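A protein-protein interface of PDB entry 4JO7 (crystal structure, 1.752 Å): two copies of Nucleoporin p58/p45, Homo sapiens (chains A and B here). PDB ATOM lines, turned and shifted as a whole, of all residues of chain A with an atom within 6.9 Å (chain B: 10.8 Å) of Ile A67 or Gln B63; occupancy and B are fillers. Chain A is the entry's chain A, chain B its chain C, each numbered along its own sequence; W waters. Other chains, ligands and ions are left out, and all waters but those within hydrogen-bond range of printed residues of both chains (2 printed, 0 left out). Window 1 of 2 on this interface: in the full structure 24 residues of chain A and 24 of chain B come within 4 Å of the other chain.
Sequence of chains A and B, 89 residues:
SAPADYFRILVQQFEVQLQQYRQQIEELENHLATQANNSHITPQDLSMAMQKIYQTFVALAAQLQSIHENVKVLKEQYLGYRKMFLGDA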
ATOM      1  N   PHE A   7     -36.058  20.678  29.253  1.00  0.00           N
ATOM      2  CA  PHE A   7     -35.884  19.536  28.350  1.00  0.00           C
ATOM      3  C   PHE A   7     -37.236  18.871  28.077  1.00  0.00           C
ATOM      4  O   PHE A   7     -37.582  18.574  26.930  1.00  0.00           O
ATOM      5  CB  PHE A   7     -34.881  18.531  28.952  1.00  0.00           C
ATOM      6  CG  PHE A   7     -34.476  17.421  28.008  1.00  0.00           C
ATOM      7  CD1 PHE A   7     -35.291  16.314  27.827  1.00  0.00           C
ATOM      8  CD2 PHE A   7     -33.273  17.475  27.331  1.00  0.00           C
ATOM      9  CE1 PHE A   7     -34.925  15.292  26.971  1.00  0.00           C
ATOM     10  CE2 PHE A   7     -32.893  16.448  26.471  1.00  0.00           C
ATOM     11  CZ  PHE A   7     -33.724  15.357  26.290  1.00  0.00           C
ATOM     12  N   ALA A  62     -36.712  10.163  20.838  1.00  0.00           N
ATOM     13  CA  ALA A  62     -36.835   9.187  21.913  1.00  0.00           C
ATOM     14  C   ALA A  62     -35.473   8.730  22.409  1.00  0.00           C
ATOM     15  O   ALA A  62     -35.274   8.550  23.613  1.00  0.00           O
ATOM     16  CB  ALA A  62     -37.678   8.000  21.467  1.00  0.00           C
ATOM     17  N   GLN A  63     -34.525   8.538  21.495  1.00  0.00           N
ATOM     18  CA  GLN A  63     -33.190   8.104  21.889  1.00  0.00           C
ATOM     19  C   GLN A  63     -32.488   9.170  22.721  1.00  0.00           C
ATOM     20  O   GLN A  63     -31.795   8.861  23.695  1.00  0.00           O
ATOM     21  CB  GLN A  63     -32.351   7.767  20.658  1.00  0.00           C
ATOM     22  CG  GLN A  63     -32.841   6.566  19.873  1.00  0.00           C
ATOM     23  CD  GLN A  63     -31.959   6.267  18.679  1.00  0.00           C
ATOM     24  OE1 GLN A  63     -31.799   7.103  17.781  1.00  0.00           O
ATOM     25  NE2 GLN A  63     -31.369   5.081  18.665  1.00  0.00           N
ATOM     26  N   LEU A  64     -32.655  10.430  22.345  1.00  0.00           N
ATOM     27  CA  LEU A  64     -32.029  11.509  23.101  1.00  0.00           C
ATOM     28  C   LEU A  64     -32.685  11.660  24.482  1.00  0.00           C
ATOM     29  O   LEU A  64     -32.006  11.940  25.471  1.00  0.00           O
ATOM     30  CB  LEU A  64     -32.069  12.824  22.311  1.00  0.00           C
ATOM     31  CG  LEU A  64     -31.122  12.843  21.100  1.00  0.00           C
ATOM     32  CD1 LEU A  64     -31.405  14.036  20.206  1.00  0.00           C
ATOM     33  CD2 LEU A  64     -29.665  12.846  21.537  1.00  0.00           C
ATOM     34  N   GLN A  65     -33.993  11.444  24.558  1.00  0.00           N
ATOM     35  CA  GLN A  65     -34.667  11.463  25.854  1.00  0.00           C
ATOM     36  C   GLN A  65     -34.079  10.363  26.756  1.00  0.00           C
ATOM     37  O   GLN A  65     -33.808  10.589  27.941  1.00  0.00           O
ATOM     38  CB  GLN A  65     -36.182  11.302  25.680  1.00  0.00           C
ATOM     39  CG  GLN A  65     -36.992  11.534  26.958  1.00  0.00           C
ATOM     40  CD  GLN A  65     -38.468  11.816  26.684  1.00  0.00           C
ATOM     41  OE1 GLN A  65     -39.078  11.207  25.805  1.00  0.00           O
ATOM     42  NE2 GLN A  65     -39.040  12.751  27.433  1.00  0.00           N
ATOM     43  N   SER A  66     -33.849   9.179  26.197  1.00  0.00           N
ATOM     44  CA  SER A  66     -33.241   8.097  26.966  1.00  0.00           C
ATOM     45  C   SER A  66     -31.812   8.423  27.402  1.00  0.00           C
ATOM     46  O   SER A  66     -31.411   8.071  28.511  1.00  0.00           O
ATOM     47  CB  SER A  66     -33.275   6.781  26.191  1.00  0.00           C
ATOM     48  OG  SER A  66     -34.524   6.143  26.370  1.00  0.00           O
ATOM     49  N   ILE A  67     -31.038   9.085  26.541  1.00  0.00           N
ATOM     50  CA  ILE A  67     -29.697   9.519  26.934  1.00  0.00           C
ATOM     51  C   ILE A  67     -29.834  10.443  28.141  1.00  0.00           C
ATOM     52  O   ILE A  67     -29.127  10.298  29.139  1.00  0.00           O
ATOM     53  CB  ILE A  67     -28.965  10.282  25.800  1.00  0.00           C
ATOM     54  CG1 ILE A  67     -28.573   9.334  24.665  1.00  0.00           C
ATOM     55  CG2 ILE A  67     -27.739  11.001  26.339  1.00  0.00           C
ATOM     56  CD1 ILE A  67     -27.486   8.350  25.025  1.00  0.00           C
ATOM     57  N   HIS A  68     -30.761  11.396  28.049  1.00  0.00           N
ATOM     58  CA  HIS A  68     -30.961  12.366  29.124  1.00  0.00           C
ATOM     59  C   HIS A  68     -31.287  11.648  30.435  1.00  0.00           C
ATOM     60  O   HIS A  68     -30.701  11.940  31.478  1.00  0.00           O
ATOM     61  CB  HIS A  68     -32.080  13.332  28.740  1.00  0.00           C
ATOM     62  CG  HIS A  68     -32.206  14.519  29.644  1.00  0.00           C
ATOM     63  ND1 HIS A  68     -33.368  14.818  30.318  1.00  0.00           N
ATOM     64  CD2 HIS A  68     -31.326  15.498  29.961  1.00  0.00           C
ATOM     65  CE1 HIS A  68     -33.197  15.923  31.023  1.00  0.00           C
ATOM     66  NE2 HIS A  68     -31.964  16.354  30.826  1.00  0.00           N
ATOM     67  N   GLU A  69     -32.202  10.685  30.368  1.00  0.00           N
ATOM     68  CA  GLU A  69     -32.590   9.909  31.542  1.00  0.00           C
ATOM     69  C   GLU A  69     -31.431   9.094  32.099  1.00  0.00           C
ATOM     70  O   GLU A  69     -31.280   8.970  33.310  1.00  0.00           O
ATOM     71  CB  GLU A  69     -33.767   8.988  31.214  1.00  0.00           C
ATOM     72  CG  GLU A  69     -35.061   9.737  30.956  1.00  0.00           C
ATOM     73  CD  GLU A  69     -35.545  10.499  32.182  1.00  0.00           C
ATOM     74  OE1 GLU A  69     -35.661   9.880  33.262  1.00  0.00           O
ATOM     75  OE2 GLU A  69     -35.786  11.722  32.072  1.00  0.00           O
ATOM     76  N   ASN A  70     -30.613   8.525  31.220  1.00  0.00           N
ATOM     77  CA  ASN A  70     -29.466   7.757  31.676  1.00  0.00           C
ATOM     78  C   ASN A  70     -28.378   8.622  32.287  1.00  0.00           C
ATOM     79  O   ASN A  70     -27.620   8.154  33.130  1.00  0.00           O
ATOM     80  CB  ASN A  70     -28.880   6.917  30.545  1.00  0.00           C
ATOM     81  CG  ASN A  70     -28.994   5.429  30.809  1.00  0.00           C
ATOM     82  OD1 ASN A  70     -29.044   4.989  31.962  1.00  0.00           O
ATOM     83  ND2 ASN A  70     -29.028   4.644  29.740  1.00  0.00           N
ATOM     84  N   VAL A  71     -28.289   9.881  31.869  1.00  0.00           N
ATOM     85  CA  VAL A  71     -27.360  10.807  32.516  1.00  0.00           C
ATOM     86  C   VAL A  71     -27.869  11.162  33.927  1.00  0.00           C
ATOM     87  O   VAL A  71     -27.080  11.371  34.855  1.00  0.00           O
ATOM     88  CB  VAL A  71     -27.123  12.056  31.660  1.00  0.00           C
ATOM     89  CG1 VAL A  71     -26.359  13.106  32.444  1.00  0.00           C
ATOM     90  CG2 VAL A  71     -26.358  11.672  30.391  1.00  0.00           C
ATOM     91  N   LYS A  72     -29.186  11.191  34.092  1.00  0.00           N
ATOM     92  CA  LYS A  72     -29.772  11.360  35.417  1.00  0.00           C
ATOM     93  C   LYS A  72     -29.426  10.173  36.314  1.00  0.00           C
ATOM     94  O   LYS A  72     -29.089  10.350  37.481  1.00  0.00           O
ATOM     95  CB  LYS A  72     -31.291  11.508  35.337  1.00  0.00           C
ATOM     96  CG  LYS A  72     -31.785  12.765  34.643  1.00  0.00           C
ATOM     97  CD  LYS A  72     -33.306  12.838  34.727  1.00  0.00           C
ATOM     98  CE  LYS A  72     -33.870  13.993  33.902  1.00  0.00           C
ATOM     99  NZ  LYS A  72     -35.353  13.987  33.906  1.00  0.00           N
ATOM    100  N   VAL A  73     -29.537   8.963  35.775  1.00  0.00           N
ATOM    101  CA  VAL A  73     -29.130   7.760  36.501  1.00  0.00           C
ATOM    102  C   VAL A  73     -27.659   7.850  36.901  1.00  0.00           C
ATOM    103  O   VAL A  73     -27.299   7.578  38.053  1.00  0.00           O
ATOM    104  CB  VAL A  73     -29.382   6.480  35.668  1.00  0.00           C
ATOM    105  CG1 VAL A  73     -28.742   5.260  36.339  1.00  0.00           C
ATOM    106  CG2 VAL A  73     -30.872   6.268  35.454  1.00  0.00           C
ATOM    107  N   PHE B   7     -17.007   7.244  13.512  1.00  0.00           N
ATOM    108  CA  PHE B   7     -17.720   7.392  14.777  1.00  0.00           C
ATOM    109  C   PHE B   7     -17.567   6.119  15.604  1.00  0.00           C
ATOM    110  O   PHE B   7     -17.301   6.177  16.803  1.00  0.00           O
ATOM    111  CB  PHE B   7     -19.197   7.714  14.587  1.00  0.00           C
ATOM    112  CG  PHE B   7     -19.874   8.164  15.860  1.00  0.00           C
ATOM    113  CD1 PHE B   7     -20.435   7.245  16.732  1.00  0.00           C
ATOM    114  CD2 PHE B   7     -19.930   9.511  16.190  1.00  0.00           C
ATOM    115  CE1 PHE B   7     -21.048   7.661  17.902  1.00  0.00           C
ATOM    116  CE2 PHE B   7     -20.533   9.927  17.359  1.00  0.00           C
ATOM    117  CZ  PHE B   7     -21.092   8.998  18.216  1.00  0.00           C
ATOM    118  N   ARG B   8     -17.728   4.965  14.959  1.00  0.00           N
ATOM    119  CA  ARG B   8     -17.577   3.695  15.654  1.00  0.00           C
ATOM    120  C   ARG B   8     -16.139   3.525  16.157  1.00  0.00           C
ATOM    121  O   ARG B   8     -15.908   2.990  17.242  1.00  0.00           O
ATOM    122  CB  ARG B   8     -17.995   2.534  14.748  1.00  0.00           C
ATOM    123  CG  ARG B   8     -17.915   1.166  15.417  1.00  0.00           C
ATOM    124  CD  ARG B   8     -18.322   0.055  14.453  1.00  0.00           C
ATOM    125  NE  ARG B   8     -19.676   0.243  13.936  1.00  0.00           N
ATOM    126  CZ  ARG B   8     -20.778  -0.283  14.471  1.00  0.00           C
ATOM    127  NH1 ARG B   8     -20.714  -1.049  15.554  1.00  0.00           N
ATOM    128  NH2 ARG B   8     -21.955  -0.043  13.912  1.00  0.00           N
ATOM    129  N   VAL B  11     -15.972   5.526  19.339  1.00  0.00           N
ATOM    130  CA  VAL B  11     -16.666   4.846  20.427  1.00  0.00           C
ATOM    131  C   VAL B  11     -15.823   3.682  20.961  1.00  0.00           C
ATOM    132  O   VAL B  11     -15.716   3.489  22.166  1.00  0.00           O
ATOM    133  CB  VAL B  11     -18.061   4.345  20.010  1.00  0.00           C
ATOM    134  CG1 VAL B  11     -18.690   3.526  21.138  1.00  0.00           C
ATOM    135  CG2 VAL B  11     -18.963   5.521  19.653  1.00  0.00           C
ATOM    136  N   PHE B  14     -13.245   4.998  23.175  1.00  0.00           N
ATOM    137  CA  PHE B  14     -13.825   5.397  24.453  1.00  0.00           C
ATOM    138  C   PHE B  14     -14.015   4.160  25.324  1.00  0.00           C
ATOM    139  O   PHE B  14     -13.716   4.173  26.522  1.00  0.00           O
ATOM    140  CB  PHE B  14     -15.155   6.127  24.240  1.00  0.00           C
ATOM    141  CG  PHE B  14     -15.824   6.545  25.515  1.00  0.00           C
ATOM    142  CD1 PHE B  14     -15.445   7.707  26.159  1.00  0.00           C
ATOM    143  CD2 PHE B  14     -16.820   5.769  26.078  1.00  0.00           C
ATOM    144  CE1 PHE B  14     -16.059   8.097  27.337  1.00  0.00           C
ATOM    145  CE2 PHE B  14     -17.437   6.155  27.259  1.00  0.00           C
ATOM    146  CZ  PHE B  14     -17.053   7.320  27.880  1.00  0.00           C
ATOM    147  N   GLU B  15     -14.479   3.078  24.716  1.00  0.00           N
ATOM    148  CA  GLU B  15     -14.742   1.849  25.452  1.00  0.00           C
ATOM    149  C   GLU B  15     -13.458   1.222  26.007  1.00  0.00           C
ATOM    150  O   GLU B  15     -13.458   0.676  27.110  1.00  0.00           O
ATOM    151  CB  GLU B  15     -15.533   0.869  24.577  1.00  0.00           C
ATOM    152  CG  GLU B  15     -16.943   1.389  24.285  1.00  0.00           C
ATOM    153  CD  GLU B  15     -17.750   0.519  23.339  1.00  0.00           C
ATOM    154  OE1 GLU B  15     -17.156  -0.229  22.537  1.00  0.00           O
ATOM    155  OE2 GLU B  15     -18.997   0.595  23.395  1.00  0.00           O
ATOM    156  N   LEU B  18     -12.555   3.215  29.008  1.00  0.00           N
ATOM    157  CA  LEU B  18     -13.330   2.770  30.169  1.00  0.00           C
ATOM    158  C   LEU B  18     -12.626   1.630  30.875  1.00  0.00           C
ATOM    159  O   LEU B  18     -12.513   1.624  32.098  1.00  0.00           O
ATOM    160  CB  LEU B  18     -14.729   2.304  29.776  1.00  0.00           C
ATOM    161  CG  LEU B  18     -15.724   3.394  29.377  1.00  0.00           C
ATOM    162  CD1 LEU B  18     -17.090   2.772  29.106  1.00  0.00           C
ATOM    163  CD2 LEU B  18     -15.811   4.482  30.434  1.00  0.00           C
ATOM    164  N   GLN B  55     -20.904   0.563  34.356  1.00  0.00           N
ATOM    165  CA  GLN B  55     -21.902  -0.089  33.522  1.00  0.00           C
ATOM    166  C   GLN B  55     -22.842   0.933  32.876  1.00  0.00           C
ATOM    167  O   GLN B  55     -23.327   0.728  31.764  1.00  0.00           O
ATOM    168  CB  GLN B  55     -22.679  -1.134  34.319  1.00  0.00           C
ATOM    169  CG  GLN B  55     -21.790  -2.310  34.798  1.00  0.00           C
ATOM    170  CD  GLN B  55     -20.963  -2.912  33.669  1.00  0.00           C
ATOM    171  OE1 GLN B  55     -19.748  -2.703  33.587  1.00  0.00           O
ATOM    172  NE2 GLN B  55     -21.617  -3.661  32.786  1.00  0.00           N
ATOM    173  N   THR B  56     -23.093   2.036  33.570  1.00  0.00           N
ATOM    174  CA  THR B  56     -23.874   3.125  32.999  1.00  0.00           C
ATOM    175  C   THR B  56     -23.092   3.820  31.884  1.00  0.00           C
ATOM    176  O   THR B  56     -23.672   4.145  30.853  1.00  0.00           O
ATOM    177  CB  THR B  56     -24.328   4.125  34.076  1.00  0.00           C
ATOM    178  OG1 THR B  56     -25.113   3.429  35.044  1.00  0.00           O
ATOM    179  CG2 THR B  56     -25.173   5.240  33.467  1.00  0.00           C
ATOM    180  N   PHE B  57     -21.781   4.007  32.062  1.00  0.00           N
ATOM    181  CA  PHE B  57     -20.950   4.551  30.984  1.00  0.00           C
ATOM    182  C   PHE B  57     -20.984   3.648  29.750  1.00  0.00           C
ATOM    183  O   PHE B  57     -21.063   4.135  28.621  1.00  0.00           O
ATOM    184  CB  PHE B  57     -19.506   4.755  31.430  1.00  0.00           C
ATOM    185  CG  PHE B  57     -19.262   6.062  32.122  1.00  0.00           C
ATOM    186  CD1 PHE B  57     -19.223   7.245  31.399  1.00  0.00           C
ATOM    187  CD2 PHE B  57     -19.078   6.115  33.494  1.00  0.00           C
ATOM    188  CE1 PHE B  57     -18.996   8.449  32.027  1.00  0.00           C
ATOM    189  CE2 PHE B  57     -18.848   7.325  34.130  1.00  0.00           C
ATOM    190  CZ  PHE B  57     -18.808   8.493  33.394  1.00  0.00           C
ATOM    191  N   VAL B  58     -20.916   2.338  29.975  1.00  0.00           N
ATOM    192  CA  VAL B  58     -21.014   1.353  28.894  1.00  0.00           C
ATOM    193  C   VAL B  58     -22.339   1.514  28.132  1.00  0.00           C
ATOM    194  O   VAL B  58     -22.364   1.559  26.894  1.00  0.00           O
ATOM    195  CB  VAL B  58     -20.870  -0.094  29.456  1.00  0.00           C
ATOM    196  CG1 VAL B  58     -21.295  -1.135  28.434  1.00  0.00           C
ATOM    197  CG2 VAL B  58     -19.424  -0.357  29.904  1.00  0.00           C
ATOM    198  N   ALA B  59     -23.436   1.612  28.876  1.00  0.00           N
ATOM    199  CA  ALA B  59     -24.761   1.780  28.290  1.00  0.00           C
ATOM    200  C   ALA B  59     -24.837   3.081  27.486  1.00  0.00           C
ATOM    201  O   ALA B  59     -25.338   3.091  26.366  1.00  0.00           O
ATOM    202  CB  ALA B  59     -25.830   1.760  29.379  1.00  0.00           C
ATOM    203  N   LEU B  60     -24.309   4.162  28.053  1.00  0.00           N
ATOM    204  CA  LEU B  60     -24.353   5.475  27.409  1.00  0.00           C
ATOM    205  C   LEU B  60     -23.601   5.493  26.080  1.00  0.00           C
ATOM    206  O   LEU B  60     -24.107   6.003  25.079  1.00  0.00           O
ATOM    207  CB  LEU B  60     -23.786   6.547  28.343  1.00  0.00           C
ATOM    208  CG  LEU B  60     -24.802   7.076  29.366  1.00  0.00           C
ATOM    209  CD1 LEU B  60     -24.102   7.825  30.481  1.00  0.00           C
ATOM    210  CD2 LEU B  60     -25.837   7.963  28.687  1.00  0.00           C
ATOM    211  N   ALA B  61     -22.394   4.938  26.075  1.00  0.00           N
ATOM    212  CA  ALA B  61     -21.587   4.886  24.860  1.00  0.00           C
ATOM    213  C   ALA B  61     -22.276   4.060  23.774  1.00  0.00           C
ATOM    214  O   ALA B  61     -22.294   4.446  22.608  1.00  0.00           O
ATOM    215  CB  ALA B  61     -20.207   4.316  25.170  1.00  0.00           C
ATOM    216  N   ALA B  62     -22.849   2.923  24.147  1.00  0.00           N
ATOM    217  CA  ALA B  62     -23.564   2.094  23.180  1.00  0.00           C
ATOM    218  C   ALA B  62     -24.808   2.804  22.636  1.00  0.00           C
ATOM    219  O   ALA B  62     -25.143   2.678  21.452  1.00  0.00           O
ATOM    220  CB  ALA B  62     -23.938   0.756  23.799  1.00  0.00           C
ATOM    221  N   GLN B  63     -25.495   3.551  23.494  1.00  0.00           N
ATOM    222  CA  GLN B  63     -26.668   4.308  23.068  1.00  0.00           C
ATOM    223  C   GLN B  63     -26.291   5.456  22.125  1.00  0.00           C
ATOM    224  O   GLN B  63     -27.015   5.740  21.165  1.00  0.00           O
ATOM    225  CB  GLN B  63     -27.478   4.797  24.277  1.00  0.00           C
ATOM    226  CG  GLN B  63     -28.241   3.652  24.947  1.00  0.00           C
ATOM    227  CD  GLN B  63     -28.876   4.027  26.270  1.00  0.00           C
ATOM    228  OE1 GLN B  63     -28.545   5.046  26.864  1.00  0.00           O
ATOM    229  NE2 GLN B  63     -29.799   3.191  26.739  1.00  0.00           N
ATOM    230  N   LEU B  64     -25.152   6.091  22.375  1.00  0.00           N
ATOM    231  CA  LEU B  64     -24.655   7.117  21.468  1.00  0.00           C
ATOM    232  C   LEU B  64     -24.340   6.525  20.093  1.00  0.00           C
ATOM    233  O   LEU B  64     -24.662   7.128  19.067  1.00  0.00           O
ATOM    234  CB  LEU B  64     -23.426   7.812  22.051  1.00  0.00           C
ATOM    235  CG  LEU B  64     -23.717   8.756  23.228  1.00  0.00           C
ATOM    236  CD1 LEU B  64     -22.444   9.395  23.744  1.00  0.00           C
ATOM    237  CD2 LEU B  64     -24.720   9.830  22.827  1.00  0.00           C
ATOM    238  N   GLN B  65     -23.730   5.343  20.070  1.00  0.00           N
ATOM    239  CA  GLN B  65     -23.495   4.652  18.800  1.00  0.00           C
ATOM    240  C   GLN B  65     -24.824   4.405  18.079  1.00  0.00           C
ATOM    241  O   GLN B  65     -24.906   4.562  16.865  1.00  0.00           O
ATOM    242  CB  GLN B  65     -22.742   3.340  19.019  1.00  0.00           C
ATOM    243  CG  GLN B  65     -22.634   2.456  17.786  1.00  0.00           C
ATOM    244  CD  GLN B  65     -21.695   3.020  16.737  1.00  0.00           C
ATOM    245  OE1 GLN B  65     -20.733   3.715  17.059  1.00  0.00           O
ATOM    246  NE2 GLN B  65     -21.965   2.710  15.473  1.00  0.00           N
ATOM    247  N   SER B  66     -25.868   4.038  18.821  1.00  0.00           N
ATOM    248  CA  SER B  66     -27.158   3.738  18.208  1.00  0.00           C
ATOM    249  C   SER B  66     -27.842   4.997  17.658  1.00  0.00           C
ATOM    250  O   SER B  66     -28.606   4.932  16.693  1.00  0.00           O
ATOM    251  CB  SER B  66     -28.076   2.982  19.177  1.00  0.00           C
ATOM    252  OG  SER B  66     -28.635   3.816  20.183  1.00  0.00           O
ATOM    253  N   ILE B  67     -27.552   6.146  18.258  1.00  0.00           N
ATOM    254  CA  ILE B  67     -28.093   7.412  17.772  1.00  0.00           C
ATOM    255  C   ILE B  67     -27.378   7.818  16.485  1.00  0.00           C
ATOM    256  O   ILE B  67     -28.017   8.205  15.483  1.00  0.00           O
ATOM    257  CB  ILE B  67     -27.958   8.504  18.847  1.00  0.00           C
ATOM    258  CG1 ILE B  67     -28.974   8.242  19.964  1.00  0.00           C
ATOM    259  CG2 ILE B  67     -28.195   9.888  18.255  1.00  0.00           C
ATOM    260  CD1 ILE B  67     -28.736   9.047  21.235  1.00  0.00           C
ATOM    261  N   HIS B  68     -26.052   7.715  16.502  1.00  0.00           N
ATOM    262  CA  HIS B  68     -25.255   7.927  15.293  1.00  0.00           C
ATOM    263  C   HIS B  68     -25.740   7.055  14.137  1.00  0.00           C
ATOM    264  O   HIS B  68     -25.847   7.532  13.005  1.00  0.00           O
ATOM    265  CB  HIS B  68     -23.780   7.641  15.563  1.00  0.00           C
ATOM    266  CG  HIS B  68     -22.973   7.446  14.320  1.00  0.00           C
ATOM    267  ND1 HIS B  68     -22.600   8.495  13.508  1.00  0.00           N
ATOM    268  CD2 HIS B  68     -22.480   6.325  13.740  1.00  0.00           C
ATOM    269  CE1 HIS B  68     -21.903   8.030  12.486  1.00  0.00           C
ATOM    270  NE2 HIS B  68     -21.814   6.718  12.604  1.00  0.00           N
ATOM    271  N   GLU B  69     -26.045   5.786  14.406  1.00  0.00           N
ATOM    272  CA  GLU B  69     -26.566   4.917  13.350  1.00  0.00           C
ATOM    273  C   GLU B  69     -27.850   5.491  12.741  1.00  0.00           C
ATOM    274  O   GLU B  69     -28.074   5.378  11.535  1.00  0.00           O
ATOM    275  CB  GLU B  69     -26.833   3.504  13.866  1.00  0.00           C
ATOM    276  CG  GLU B  69     -25.571   2.708  14.185  1.00  0.00           C
ATOM    277  CD  GLU B  69     -24.659   2.535  12.985  1.00  0.00           C
ATOM    278  OE1 GLU B  69     -25.161   2.562  11.842  1.00  0.00           O
ATOM    279  OE2 GLU B  69     -23.436   2.375  13.189  1.00  0.00           O
ATOM    280  N   ASN B  70     -28.702   6.091  13.565  1.00  0.00           N
ATOM    281  CA  ASN B  70     -29.912   6.714  13.033  1.00  0.00           C
ATOM    282  C   ASN B  70     -29.639   8.020  12.287  1.00  0.00           C
ATOM    283  O   ASN B  70     -30.355   8.355  11.347  1.00  0.00           O
ATOM    284  CB  ASN B  70     -30.968   6.912  14.122  1.00  0.00           C
ATOM    285  CG  ASN B  70     -31.867   5.699  14.286  1.00  0.00           C
ATOM    286  OD1 ASN B  70     -31.994   4.882  13.378  1.00  0.00           O
ATOM    287  ND2 ASN B  70     -32.509   5.588  15.438  1.00  0.00           N
ATOM    288  N   VAL B  71     -28.601   8.751  12.679  1.00  0.00           N
ATOM    289  CA  VAL B  71     -28.208   9.930  11.913  1.00  0.00           C
ATOM    290  C   VAL B  71     -27.720   9.493  10.531  1.00  0.00           C
ATOM    291  O   VAL B  71     -27.979  10.167   9.527  1.00  0.00           O
ATOM    292  CB  VAL B  71     -27.117  10.752  12.634  1.00  0.00           C
ATOM    293  CG1 VAL B  71     -26.609  11.879  11.740  1.00  0.00           C
ATOM    294  CG2 VAL B  71     -27.663  11.314  13.939  1.00  0.00           C
HETATM  295  O   HOH W   1     -31.909   3.095  28.554  1.00  0.00           O
HETATM  296  O   HOH W   2     -27.623   2.823  33.671  1.00  0.00           O
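The side-chain amide nitrogen of Gln A63 lies within hydrogen-bond range of the side-chain hydroxyl of Ser B66, 3.4 Å away. ND2 of Asn B70 sits at hydrogen-bond distance from OE1 of Gln A63, at 2.9 Å. ND2 of Asn A70 is in hydrogen-bond range of OE1 of Gln B63.
The backbone carbonyl oxygen (O) of Gln B63 is in hydrogen-bond range of the side-chain hydroxyl (OG) of Ser B66 (2.7 Å).
Among the printed residues, pairs that only touch across the chains: Ile A67 with Ile B67 (3.4 Å), Gln A63 with Ile B67 (3.5 Å), Ile A67 with Gln B63 (3.6 Å), Asn A70 with Leu B60 (3.7 Å), Asn A70 with Thr B56 (3.8 Å), Ile A67 with Leu B64 (3.8 Å) and Leu A64 with Ile B67 (3.9 Å).
Of chain B, only Ser B66, Ile B67 and Asn B70 come within 4 Å of Gln A63. Ile A67 touches just these residues of chain B: Gln B63, Leu B64 and Ile B67. Printed residues of chain B within 4 Å of Asn A70: Thr B56, Leu B60 and Gln B63. Of the printed residues of chain A, Leu B60 touches Asn A70 (3.7 Å). Of the printed residues of chain A, Gln B63 touches Ile A67 and Asn A70. Of the printed residues of chain A, Leu B64 touches Ile A67. Printed residues of chain A within 4 Å of Asn B70: Gln A63 (2.9 Å). The nearest residue of chain B that does not touch Ile A67 is Leu B60 (4.03 Å). The nearest printed residue of chain A that does not touch Gln B63 is Ser A66 (4.5 Å). The nearest printed residue of chain A that does not touch Thr B56 is Val A73 (4.3 Å).
Of the 23 printed residues of chain B, 7 touch a printed residue of chain A. Of the 13 printed residues of chain A, 4 touch a printed residue of chain B. Hydrophobic or aromatic side chains of chain A within 4 Å of the printed part of chain B: Leu A64 and Ile A67. Along chain A the printed residues that touch a printed residue of chain B span positions 63 to 70. Among the printed residues, 10 pairs touch across the chains.
Gln A63 touches Ser B66, but with the chains exchanged Ser A66 does not touch Gln B63 (4.5 Å). Gln A63 touches Ile B67, and with the chains exchanged Ile A67 touches Gln B63. Leu A64 touches Ile B67, and with the chains exchanged Ile A67 touches Leu B64. Ile A67 touches its own counterpart, Ile B67.
Water W1 lies within hydrogen-bond range of NE2 of Gln B63 (2.8 Å) and ND2 of Asn A70 (3.5 Å). Water W2 lies within hydrogen-bond range of OG1 of Thr B56 (2.9 Å) and OD1 of Asn A70 (3.1 Å).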
